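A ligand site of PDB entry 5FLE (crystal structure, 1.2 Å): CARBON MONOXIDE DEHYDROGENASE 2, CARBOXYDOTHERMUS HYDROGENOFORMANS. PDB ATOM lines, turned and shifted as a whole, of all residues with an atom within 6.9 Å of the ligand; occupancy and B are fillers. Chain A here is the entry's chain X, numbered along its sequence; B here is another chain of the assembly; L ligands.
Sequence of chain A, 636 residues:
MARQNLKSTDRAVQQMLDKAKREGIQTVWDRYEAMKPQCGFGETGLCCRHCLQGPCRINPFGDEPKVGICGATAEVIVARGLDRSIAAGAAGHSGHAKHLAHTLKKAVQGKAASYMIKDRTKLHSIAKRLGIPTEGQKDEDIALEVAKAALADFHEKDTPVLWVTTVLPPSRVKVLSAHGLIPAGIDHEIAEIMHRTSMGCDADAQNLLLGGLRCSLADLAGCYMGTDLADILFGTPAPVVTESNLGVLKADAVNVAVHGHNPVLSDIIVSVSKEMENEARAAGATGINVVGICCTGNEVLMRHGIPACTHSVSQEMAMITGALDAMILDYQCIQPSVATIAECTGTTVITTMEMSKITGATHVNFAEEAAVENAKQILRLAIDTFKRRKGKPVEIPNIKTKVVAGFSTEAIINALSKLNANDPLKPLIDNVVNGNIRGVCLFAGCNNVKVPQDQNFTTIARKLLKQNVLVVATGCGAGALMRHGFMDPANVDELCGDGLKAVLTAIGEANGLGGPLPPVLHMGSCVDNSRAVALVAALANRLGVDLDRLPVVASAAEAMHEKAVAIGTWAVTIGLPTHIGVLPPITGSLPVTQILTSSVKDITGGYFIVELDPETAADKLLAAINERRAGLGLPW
N of Cys 51 sits close to S1 of the ligand. SG of Cys 51 binds FE3 of the ligand (2.3 Å). SG of Cys 56 binds FE4 of the ligand (2.3 Å). SG of Cys 48 is bound to FE2 of the ligand. A sulfur (S2) of the ligand sits close to the backbone NH (N) of Cys 70. FE1 of the ligand is bound by SG of Cys 70 (2.3 Å). NH2 of Arg 80 lies close to S4 of the ligand. N of Gly 54 lies close to S1 of the ligand, at 3.7 Å. The side-chain amide nitrogen of Gln 53 lies close to a sulfur (S2) of the ligand (3.7 Å). The backbone NH (N) of His 50 lies close to a sulfur (S1) of the ligand (3.8 Å).
The side-chain sulfur of Cys 51 lies close to the side-chain sulfur of Met 560 of chain B (3.7 Å). The backbone carbonyl oxygen of Cys 56 is in hydrogen-bond range of the backbone NH of Cys 48 (2.8 Å). The side-chain sulfur (SG) of Cys 56 lies close to the backbone NH (N) of Ile 69 (3.4 Å). The backbone carbonyl oxygen (O) of Cys 56 sits close to the side-chain sulfur (SG) of Cys 47 (3.6 Å). The guanidinium group (NH2) of Arg 80 sits close to the side-chain sulfur (SG) of Cys 48 (3.4 Å). SG of Cys 48 sits close to N of His 50, at 3.4 Å. The side-chain sulfur of Cys 70 lies close to the backbone NH of Ala 72 (3.5 Å). A ring nitrogen (ND1) of His 50 lies within hydrogen-bond range of the backbone carbonyl oxygen (O) of Thr 197 (2.8 Å).
Merely in contact with the ligand: Met 199, Ile 69, Gly 68 and Ala 72. Hydrophobic or aromatic side chains within 4 Å of the ligand: Ile 69, Ala 72 and Met 199. Within 4 Å of the ligand: Cys 48, His 50, Cys 51, Gln 53, Gly 54, Cys 56, Gly 68, Ile 69, Cys 70, Ala 72, Arg 80 and Met 199.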
ATOM      1  N   CYS A  47      15.087 -13.322 -17.960  1.00  0.00           N
ATOM      2  CA  CYS A  47      15.367 -12.628 -16.694  1.00  0.00           C
ATOM      3  C   CYS A  47      15.680 -11.204 -17.053  1.00  0.00           C
ATOM      4  O   CYS A  47      16.395 -10.925 -18.025  1.00  0.00           O
ATOM      5  CB  CYS A  47      16.485 -13.278 -15.924  1.00  0.00           C
ATOM      6  SG  CYS A  47      16.860 -12.401 -14.378  1.00  0.00           S
ATOM      7  N   CYS A  48      15.170 -10.282 -16.228  1.00  0.00           N
ATOM      8  CA  CYS A  48      15.455  -8.864 -16.335  1.00  0.00           C
ATOM      9  C   CYS A  48      15.755  -8.295 -14.949  1.00  0.00           C
ATOM     10  O   CYS A  48      14.977  -8.493 -13.997  1.00  0.00           O
ATOM     11  CB  CYS A  48      14.259  -8.140 -16.967  1.00  0.00           C
ATOM     12  SG  CYS A  48      14.538  -6.367 -17.204  1.00  0.00           S
ATOM     13  N   ARG A  49      16.843  -7.510 -14.901  1.00  0.00           N
ATOM     14  CA  ARG A  49      17.246  -6.731 -13.731  1.00  0.00           C
ATOM     15  C   ARG A  49      17.449  -5.254 -14.088  1.00  0.00           C
ATOM     16  O   ARG A  49      18.258  -4.568 -13.503  1.00  0.00           O
ATOM     17  CB  ARG A  49      18.508  -7.336 -13.082  1.00  0.00           C
ATOM     18  CG  ARG A  49      18.298  -8.719 -12.581  1.00  0.00           C
ATOM     19  CD  ARG A  49      19.591  -9.379 -12.217  1.00  0.00           C
ATOM     20  NE  ARG A  49      20.292  -8.653 -11.227  1.00  0.00           N
ATOM     21  CZ  ARG A  49      21.601  -8.652 -11.000  1.00  0.00           C
ATOM     22  NH1 ARG A  49      22.421  -9.453 -11.701  1.00  0.00           N
ATOM     23  NH2 ARG A  49      22.104  -7.946  -9.969  1.00  0.00           N
ATOM     24  N   HIS A  50      16.694  -4.804 -15.061  1.00  0.00           N
ATOM     25  CA  HIS A  50      16.895  -3.400 -15.515  1.00  0.00           C
ATOM     26  C   HIS A  50      16.226  -2.362 -14.629  1.00  0.00           C
ATOM     27  O   HIS A  50      16.444  -1.173 -14.886  1.00  0.00           O
ATOM     28  CB  HIS A  50      16.476  -3.207 -16.959  1.00  0.00           C
ATOM     29  CG  HIS A  50      17.296  -3.979 -17.957  1.00  0.00           C
ATOM     30  ND1 HIS A  50      17.214  -3.696 -19.307  1.00  0.00           N
ATOM     31  CD2 HIS A  50      18.145  -5.036 -17.833  1.00  0.00           C
ATOM     32  CE1 HIS A  50      18.045  -4.527 -19.946  1.00  0.00           C
ATOM     33  NE2 HIS A  50      18.606  -5.355 -19.093  1.00  0.00           N
ATOM     34  N   CYS A  51      15.570  -2.749 -13.539  1.00  0.00           N
ATOM     35  CA  CYS A  51      15.172  -1.753 -12.534  1.00  0.00           C
ATOM     36  C   CYS A  51      15.066  -2.450 -11.214  1.00  0.00           C
ATOM     37  O   CYS A  51      15.124  -3.675 -11.086  1.00  0.00           O
ATOM     38  CB  CYS A  51      13.892  -1.009 -12.914  1.00  0.00           C
ATOM     39  SG  CYS A  51      12.327  -1.926 -12.564  1.00  0.00           S
ATOM     40  N   LEU A  52      14.889  -1.646 -10.160  1.00  0.00           N
ATOM     41  CA  LEU A  52      14.857  -2.108  -8.798  1.00  0.00           C
ATOM     42  C   LEU A  52      13.521  -2.705  -8.354  1.00  0.00           C
ATOM     43  O   LEU A  52      13.385  -3.097  -7.201  1.00  0.00           O
ATOM     44  CB  LEU A  52      15.353  -1.046  -7.815  1.00  0.00           C
ATOM     45  CG  LEU A  52      16.706  -0.437  -8.046  1.00  0.00           C
ATOM     46  CD1 LEU A  52      17.000   0.563  -6.951  1.00  0.00           C
ATOM     47  CD2 LEU A  52      17.764  -1.533  -8.045  1.00  0.00           C
ATOM     48  N   GLN A  53      12.599  -2.832  -9.274  1.00  0.00           N
ATOM     49  CA  GLN A  53      11.442  -3.658  -9.035  1.00  0.00           C
ATOM     50  C   GLN A  53      11.724  -5.135  -9.255  1.00  0.00           C
ATOM     51  O   GLN A  53      10.986  -5.968  -8.791  1.00  0.00           O
ATOM     52  CB  GLN A  53      10.230  -3.245  -9.866  1.00  0.00           C
ATOM     53  CG  GLN A  53       9.718  -1.877  -9.469  1.00  0.00           C
ATOM     54  CD  GLN A  53       8.588  -1.302 -10.285  1.00  0.00           C
ATOM     55  OE1 GLN A  53       7.732  -0.611  -9.703  1.00  0.00           O
ATOM     56  NE2 GLN A  53       8.502  -1.553 -11.552  1.00  0.00           N
ATOM     57  N   GLY A  54      12.814  -5.401 -10.017  1.00  0.00           N
ATOM     58  CA  GLY A  54      13.157  -6.818 -10.278  1.00  0.00           C
ATOM     59  C   GLY A  54      13.882  -7.387  -9.115  1.00  0.00           C
ATOM     60  O   GLY A  54      14.008  -6.817  -8.019  1.00  0.00           O
ATOM     61  N   PRO A  55      14.477  -8.577  -9.310  1.00  0.00           N
ATOM     62  CA  PRO A  55      14.538  -9.246 -10.621  1.00  0.00           C
ATOM     63  C   PRO A  55      13.200  -9.777 -11.102  1.00  0.00           C
ATOM     64  O   PRO A  55      12.394 -10.261 -10.280  1.00  0.00           O
ATOM     65  CB  PRO A  55      15.487 -10.418 -10.379  1.00  0.00           C
ATOM     66  CG  PRO A  55      16.083 -10.186  -9.097  1.00  0.00           C
ATOM     67  CD  PRO A  55      15.222  -9.314  -8.295  1.00  0.00           C
ATOM     68  N   CYS A  56      12.956  -9.698 -12.411  1.00  0.00           N
ATOM     69  CA  CYS A  56      11.837 -10.329 -13.026  1.00  0.00           C
ATOM     70  C   CYS A  56      12.289 -11.501 -13.826  1.00  0.00           C
ATOM     71  O   CYS A  56      13.353 -11.484 -14.462  1.00  0.00           O
ATOM     72  CB  CYS A  56      11.149  -9.307 -13.971  1.00  0.00           C
ATOM     73  SG  CYS A  56      10.298  -7.966 -13.027  1.00  0.00           S
ATOM     74  N   ARG A  57      11.486 -12.543 -13.839  1.00  0.00           N
ATOM     75  CA  ARG A  57      11.699 -13.705 -14.683  1.00  0.00           C
ATOM     76  C   ARG A  57      10.398 -14.109 -15.301  1.00  0.00           C
ATOM     77  O   ARG A  57       9.306 -13.702 -14.821  1.00  0.00           O
ATOM     78  CB  ARG A  57      12.336 -14.809 -13.825  1.00  0.00           C
ATOM     79  CG  ARG A  57      11.349 -15.405 -12.875  1.00  0.00           C
ATOM     80  CD  ARG A  57      11.958 -16.271 -11.783  1.00  0.00           C
ATOM     81  NE  ARG A  57      10.859 -16.818 -10.980  1.00  0.00           N
ATOM     82  CZ  ARG A  57      10.080 -16.110 -10.133  1.00  0.00           C
ATOM     83  NH1 ARG A  57      10.289 -14.808  -9.735  1.00  0.00           N
ATOM     84  NH2 ARG A  57       9.026 -16.738  -9.625  1.00  0.00           N
ATOM     85  N   VAL A  67       4.995 -12.437 -17.445  1.00  0.00           N
ATOM     86  CA  VAL A  67       5.296 -11.094 -17.941  1.00  0.00           C
ATOM     87  C   VAL A  67       6.062 -10.382 -16.843  1.00  0.00           C
ATOM     88  O   VAL A  67       5.889 -10.661 -15.660  1.00  0.00           O
ATOM     89  CB  VAL A  67       3.967 -10.381 -18.287  1.00  0.00           C
ATOM     90  CG1 VAL A  67       3.070 -10.293 -17.097  1.00  0.00           C
ATOM     91  CG2 VAL A  67       4.200  -9.044 -18.925  1.00  0.00           C
ATOM     92  N   GLY A  68       6.908  -9.437 -17.231  1.00  0.00           N
ATOM     93  CA  GLY A  68       7.620  -8.641 -16.282  1.00  0.00           C
ATOM     94  C   GLY A  68       6.694  -7.710 -15.475  1.00  0.00           C
ATOM     95  O   GLY A  68       5.578  -7.393 -15.883  1.00  0.00           O
ATOM     96  N   ILE A  69       7.202  -7.230 -14.333  1.00  0.00           N
ATOM     97  CA  ILE A  69       6.364  -6.358 -13.474  1.00  0.00           C
ATOM     98  C   ILE A  69       5.865  -5.121 -14.178  1.00  0.00           C
ATOM     99  O   ILE A  69       4.685  -4.751 -14.006  1.00  0.00           O
ATOM    100  CB  ILE A  69       7.123  -6.059 -12.165  1.00  0.00           C
ATOM    101  CG1 ILE A  69       7.208  -7.329 -11.302  1.00  0.00           C
ATOM    102  CG2 ILE A  69       6.478  -4.900 -11.411  1.00  0.00           C
ATOM    103  CD1 ILE A  69       8.106  -7.242 -10.100  1.00  0.00           C
ATOM    104  N   CYS A  70       6.694  -4.496 -15.004  1.00  0.00           N
ATOM    105  CA  CYS A  70       6.279  -3.269 -15.720  1.00  0.00           C
ATOM    106  C   CYS A  70       5.444  -3.561 -16.934  1.00  0.00           C
ATOM    107  O   CYS A  70       5.011  -2.641 -17.606  1.00  0.00           O
ATOM    108  CB  CYS A  70       7.526  -2.535 -16.157  1.00  0.00           C
ATOM    109  SG  CYS A  70       8.574  -3.516 -17.272  1.00  0.00           S
ATOM    110  N   GLY A  71       5.233  -4.879 -17.218  1.00  0.00           N
ATOM    111  CA  GLY A  71       4.562  -5.285 -18.448  1.00  0.00           C
ATOM    112  C   GLY A  71       5.473  -5.759 -19.572  1.00  0.00           C
ATOM    113  O   GLY A  71       4.987  -6.103 -20.645  1.00  0.00           O
ATOM    114  N   ALA A  72       6.798  -5.752 -19.362  1.00  0.00           N
ATOM    115  CA  ALA A  72       7.746  -6.206 -20.386  1.00  0.00           C
ATOM    116  C   ALA A  72       7.459  -7.685 -20.720  1.00  0.00           C
ATOM    117  O   ALA A  72       7.486  -8.546 -19.861  1.00  0.00           O
ATOM    118  CB  ALA A  72       9.172  -6.015 -19.932  1.00  0.00           C
ATOM    119  N   THR A  73       7.258  -7.930 -22.003  1.00  0.00           N
ATOM    120  CA  THR A  73       6.997  -9.284 -22.483  1.00  0.00           C
ATOM    121  C   THR A  73       8.333 -10.092 -22.583  1.00  0.00           C
ATOM    122  O   THR A  73       9.431  -9.538 -22.550  1.00  0.00           O
ATOM    123  CB  THR A  73       6.347  -9.292 -23.834  1.00  0.00           C
ATOM    124  OG1 THR A  73       7.229  -8.646 -24.747  1.00  0.00           O
ATOM    125  CG2 THR A  73       4.952  -8.616 -23.826  1.00  0.00           C
ATOM    126  N   ILE A  77      12.077  -8.511 -23.115  1.00  0.00           N
ATOM    127  CA  ILE A  77      13.154  -8.816 -22.174  1.00  0.00           C
ATOM    128  C   ILE A  77      14.339  -9.470 -22.912  1.00  0.00           C
ATOM    129  O   ILE A  77      15.481  -9.061 -22.751  1.00  0.00           O
ATOM    130  CB  ILE A  77      12.602  -9.729 -21.049  1.00  0.00           C
ATOM    131  CG1 ILE A  77      11.719  -8.834 -20.107  1.00  0.00           C
ATOM    132  CG2 ILE A  77      13.698 -10.449 -20.307  1.00  0.00           C
ATOM    133  CD1 ILE A  77      11.001  -9.670 -19.048  1.00  0.00           C
ATOM    134  N   ARG A  80      16.093  -6.845 -25.202  1.00  0.00           N
ATOM    135  CA  ARG A  80      16.860  -5.843 -24.451  1.00  0.00           C
ATOM    136  C   ARG A  80      18.152  -6.420 -23.938  1.00  0.00           C
ATOM    137  O   ARG A  80      19.162  -5.759 -23.984  1.00  0.00           O
ATOM    138  CB  ARG A  80      16.021  -5.285 -23.300  1.00  0.00           C
ATOM    139  CG  ARG A  80      14.804  -4.464 -23.755  1.00  0.00           C
ATOM    140  CD  ARG A  80      14.121  -3.681 -22.634  1.00  0.00           C
ATOM    141  NE  ARG A  80      13.738  -4.526 -21.517  1.00  0.00           N
ATOM    142  CZ  ARG A  80      12.923  -4.126 -20.578  1.00  0.00           C
ATOM    143  NH1 ARG A  80      12.361  -2.905 -20.672  1.00  0.00           N
ATOM    144  NH2 ARG A  80      12.612  -4.911 -19.573  1.00  0.00           N
ATOM    145  N   THR A 197      17.014   0.372 -23.886  1.00  0.00           N
ATOM    146  CA  THR A 197      16.799  -0.831 -23.165  1.00  0.00           C
ATOM    147  C   THR A 197      16.523  -0.649 -21.676  1.00  0.00           C
ATOM    148  O   THR A 197      16.264  -1.638 -20.973  1.00  0.00           O
ATOM    149  CB  THR A 197      18.014  -1.814 -23.349  1.00  0.00           C
ATOM    150  OG1 THR A 197      19.178  -1.175 -22.871  1.00  0.00           O
ATOM    151  CG2 THR A 197      18.159  -2.264 -24.796  1.00  0.00           C
ATOM    152  N   SER A 198      16.661   0.581 -21.205  1.00  0.00           N
ATOM    153  CA  SER A 198      16.332   0.870 -19.810  1.00  0.00           C
ATOM    154  C   SER A 198      14.800   0.829 -19.585  1.00  0.00           C
ATOM    155  O   SER A 198      14.046   0.740 -20.518  1.00  0.00           O
ATOM    156  CB  SER A 198      16.955   2.199 -19.357  1.00  0.00           C
ATOM    157  OG  SER A 198      16.269   3.307 -19.864  1.00  0.00           O
ATOM    158  N   MET A 199      14.402   0.803 -18.336  1.00  0.00           N
ATOM    159  CA  MET A 199      12.984   0.558 -18.023  1.00  0.00           C
ATOM    160  C   MET A 199      12.084   1.598 -18.658  1.00  0.00           C
ATOM    161  O   MET A 199      12.374   2.830 -18.632  1.00  0.00           O
ATOM    162  CB  MET A 199      12.822   0.461 -16.506  1.00  0.00           C
ATOM    163  CG  MET A 199      11.376   0.209 -16.024  1.00  0.00           C
ATOM    164  SD  MET A 199      10.377   1.718 -15.996  1.00  0.00           S
ATOM    165  CE  MET A 199       8.895   1.101 -15.271  1.00  0.00           C
ATOM    166  N   GLY A 200      11.004   1.137 -19.237  1.00  0.00           N
ATOM    167  CA  GLY A 200       9.972   2.043 -19.699  1.00  0.00           C
ATOM    168  C   GLY A 200      10.333   2.835 -20.958  1.00  0.00           C
ATOM    169  O   GLY A 200       9.763   3.906 -21.172  1.00  0.00           O
ATOM    170  N   VAL B  28       0.176  -3.460 -12.467  1.00  0.00           N
ATOM    171  CA  VAL B  28       1.578  -3.635 -12.004  1.00  0.00           C
ATOM    172  C   VAL B  28       1.603  -4.401 -10.653  1.00  0.00           C
ATOM    173  O   VAL B  28       2.500  -5.211 -10.423  1.00  0.00           O
ATOM    174  CB  VAL B  28       2.276  -2.231 -11.940  1.00  0.00           C
ATOM    175  CG1 VAL B  28       1.565  -1.325 -10.890  1.00  0.00           C
ATOM    176  CG2 VAL B  28       3.727  -2.404 -11.657  1.00  0.00           C
ATOM    177  N   MET B  35       5.079 -12.458  -9.476  1.00  0.00           N
ATOM    178  CA  MET B  35       6.505 -12.623  -9.522  1.00  0.00           C
ATOM    179  C   MET B  35       7.125 -13.132  -8.223  1.00  0.00           C
ATOM    180  O   MET B  35       8.287 -13.525  -8.181  1.00  0.00           O
ATOM    181  CB  MET B  35       7.160 -11.256  -9.852  1.00  0.00           C
ATOM    182  CG  MET B  35       8.585 -11.339 -10.414  1.00  0.00           C
ATOM    183  SD  MET B  35       8.703 -12.311 -11.957  1.00  0.00           S
ATOM    184  CE  MET B  35       7.894 -11.229 -13.102  1.00  0.00           C
ATOM    185  N   GLN B  38      10.647 -13.400  -5.470  1.00  0.00           N
ATOM    186  CA  GLN B  38      11.630 -12.985  -6.429  1.00  0.00           C
ATOM    187  C   GLN B  38      12.988 -13.630  -6.173  1.00  0.00           C
ATOM    188  O   GLN B  38      13.292 -14.021  -5.069  1.00  0.00           O
ATOM    189  CB  GLN B  38      11.763 -11.448  -6.444  1.00  0.00           C
ATOM    190  CG  GLN B  38      10.500 -10.766  -6.951  1.00  0.00           C
ATOM    191  CD  GLN B  38      10.577  -9.294  -7.050  1.00  0.00           C
ATOM    192  OE1 GLN B  38      10.397  -8.609  -6.066  1.00  0.00           O
ATOM    193  NE2 GLN B  38      10.917  -8.796  -8.203  1.00  0.00           N
ATOM    194  N   PRO B 336       5.155  -0.707 -20.271  1.00  0.00           N
ATOM    195  CA  PRO B 336       4.639  -1.085 -21.600  1.00  0.00           C
ATOM    196  C   PRO B 336       3.280  -1.775 -21.542  1.00  0.00           C
ATOM    197  O   PRO B 336       2.615  -1.918 -22.555  1.00  0.00           O
ATOM    198  CB  PRO B 336       5.759  -1.987 -22.174  1.00  0.00           C
ATOM    199  CG  PRO B 336       6.486  -2.472 -20.957  1.00  0.00           C
ATOM    200  CD  PRO B 336       6.483  -1.338 -19.997  1.00  0.00           C
ATOM    201  N   MET B 560      13.481   3.248  -8.188  1.00  0.00           N
ATOM    202  CA  MET B 560      13.175   2.183  -9.151  1.00  0.00           C
ATOM    203  C   MET B 560      14.144   2.174 -10.324  1.00  0.00           C
ATOM    204  O   MET B 560      14.807   1.155 -10.603  1.00  0.00           O
ATOM    205  CB  MET B 560      11.695   2.252  -9.580  1.00  0.00           C
ATOM    206  CG  MET B 560      11.263   1.247 -10.626  1.00  0.00           C
ATOM    207  SD  MET B 560      11.477   1.705 -12.362  1.00  0.00           S
ATOM    208  CE  MET B 560      10.449   3.119 -12.462  1.00  0.00           C
HETATM  209 FE1  LIG L   1      10.382  -4.298 -16.086  1.00  0.00          FE
HETATM  210 FE2  LIG L   1      12.866  -5.408 -15.953  1.00  0.00          FE
HETATM  211 FE3  LIG L   1      12.163  -3.625 -14.037  1.00  0.00          FE
HETATM  212 FE4  LIG L   1      11.053  -6.101 -14.128  1.00  0.00          FE
HETATM  213  S1  LIG L   1      13.251  -5.555 -13.717  1.00  0.00           S
HETATM  214  S2  LIG L   1       9.919  -4.187 -13.804  1.00  0.00           S
HETATM  215  S3  LIG L   1      10.881  -6.480 -16.407  1.00  0.00           S
HETATM  216  S4  LIG L   1      12.422  -3.235 -16.330  1.00  0.00           S
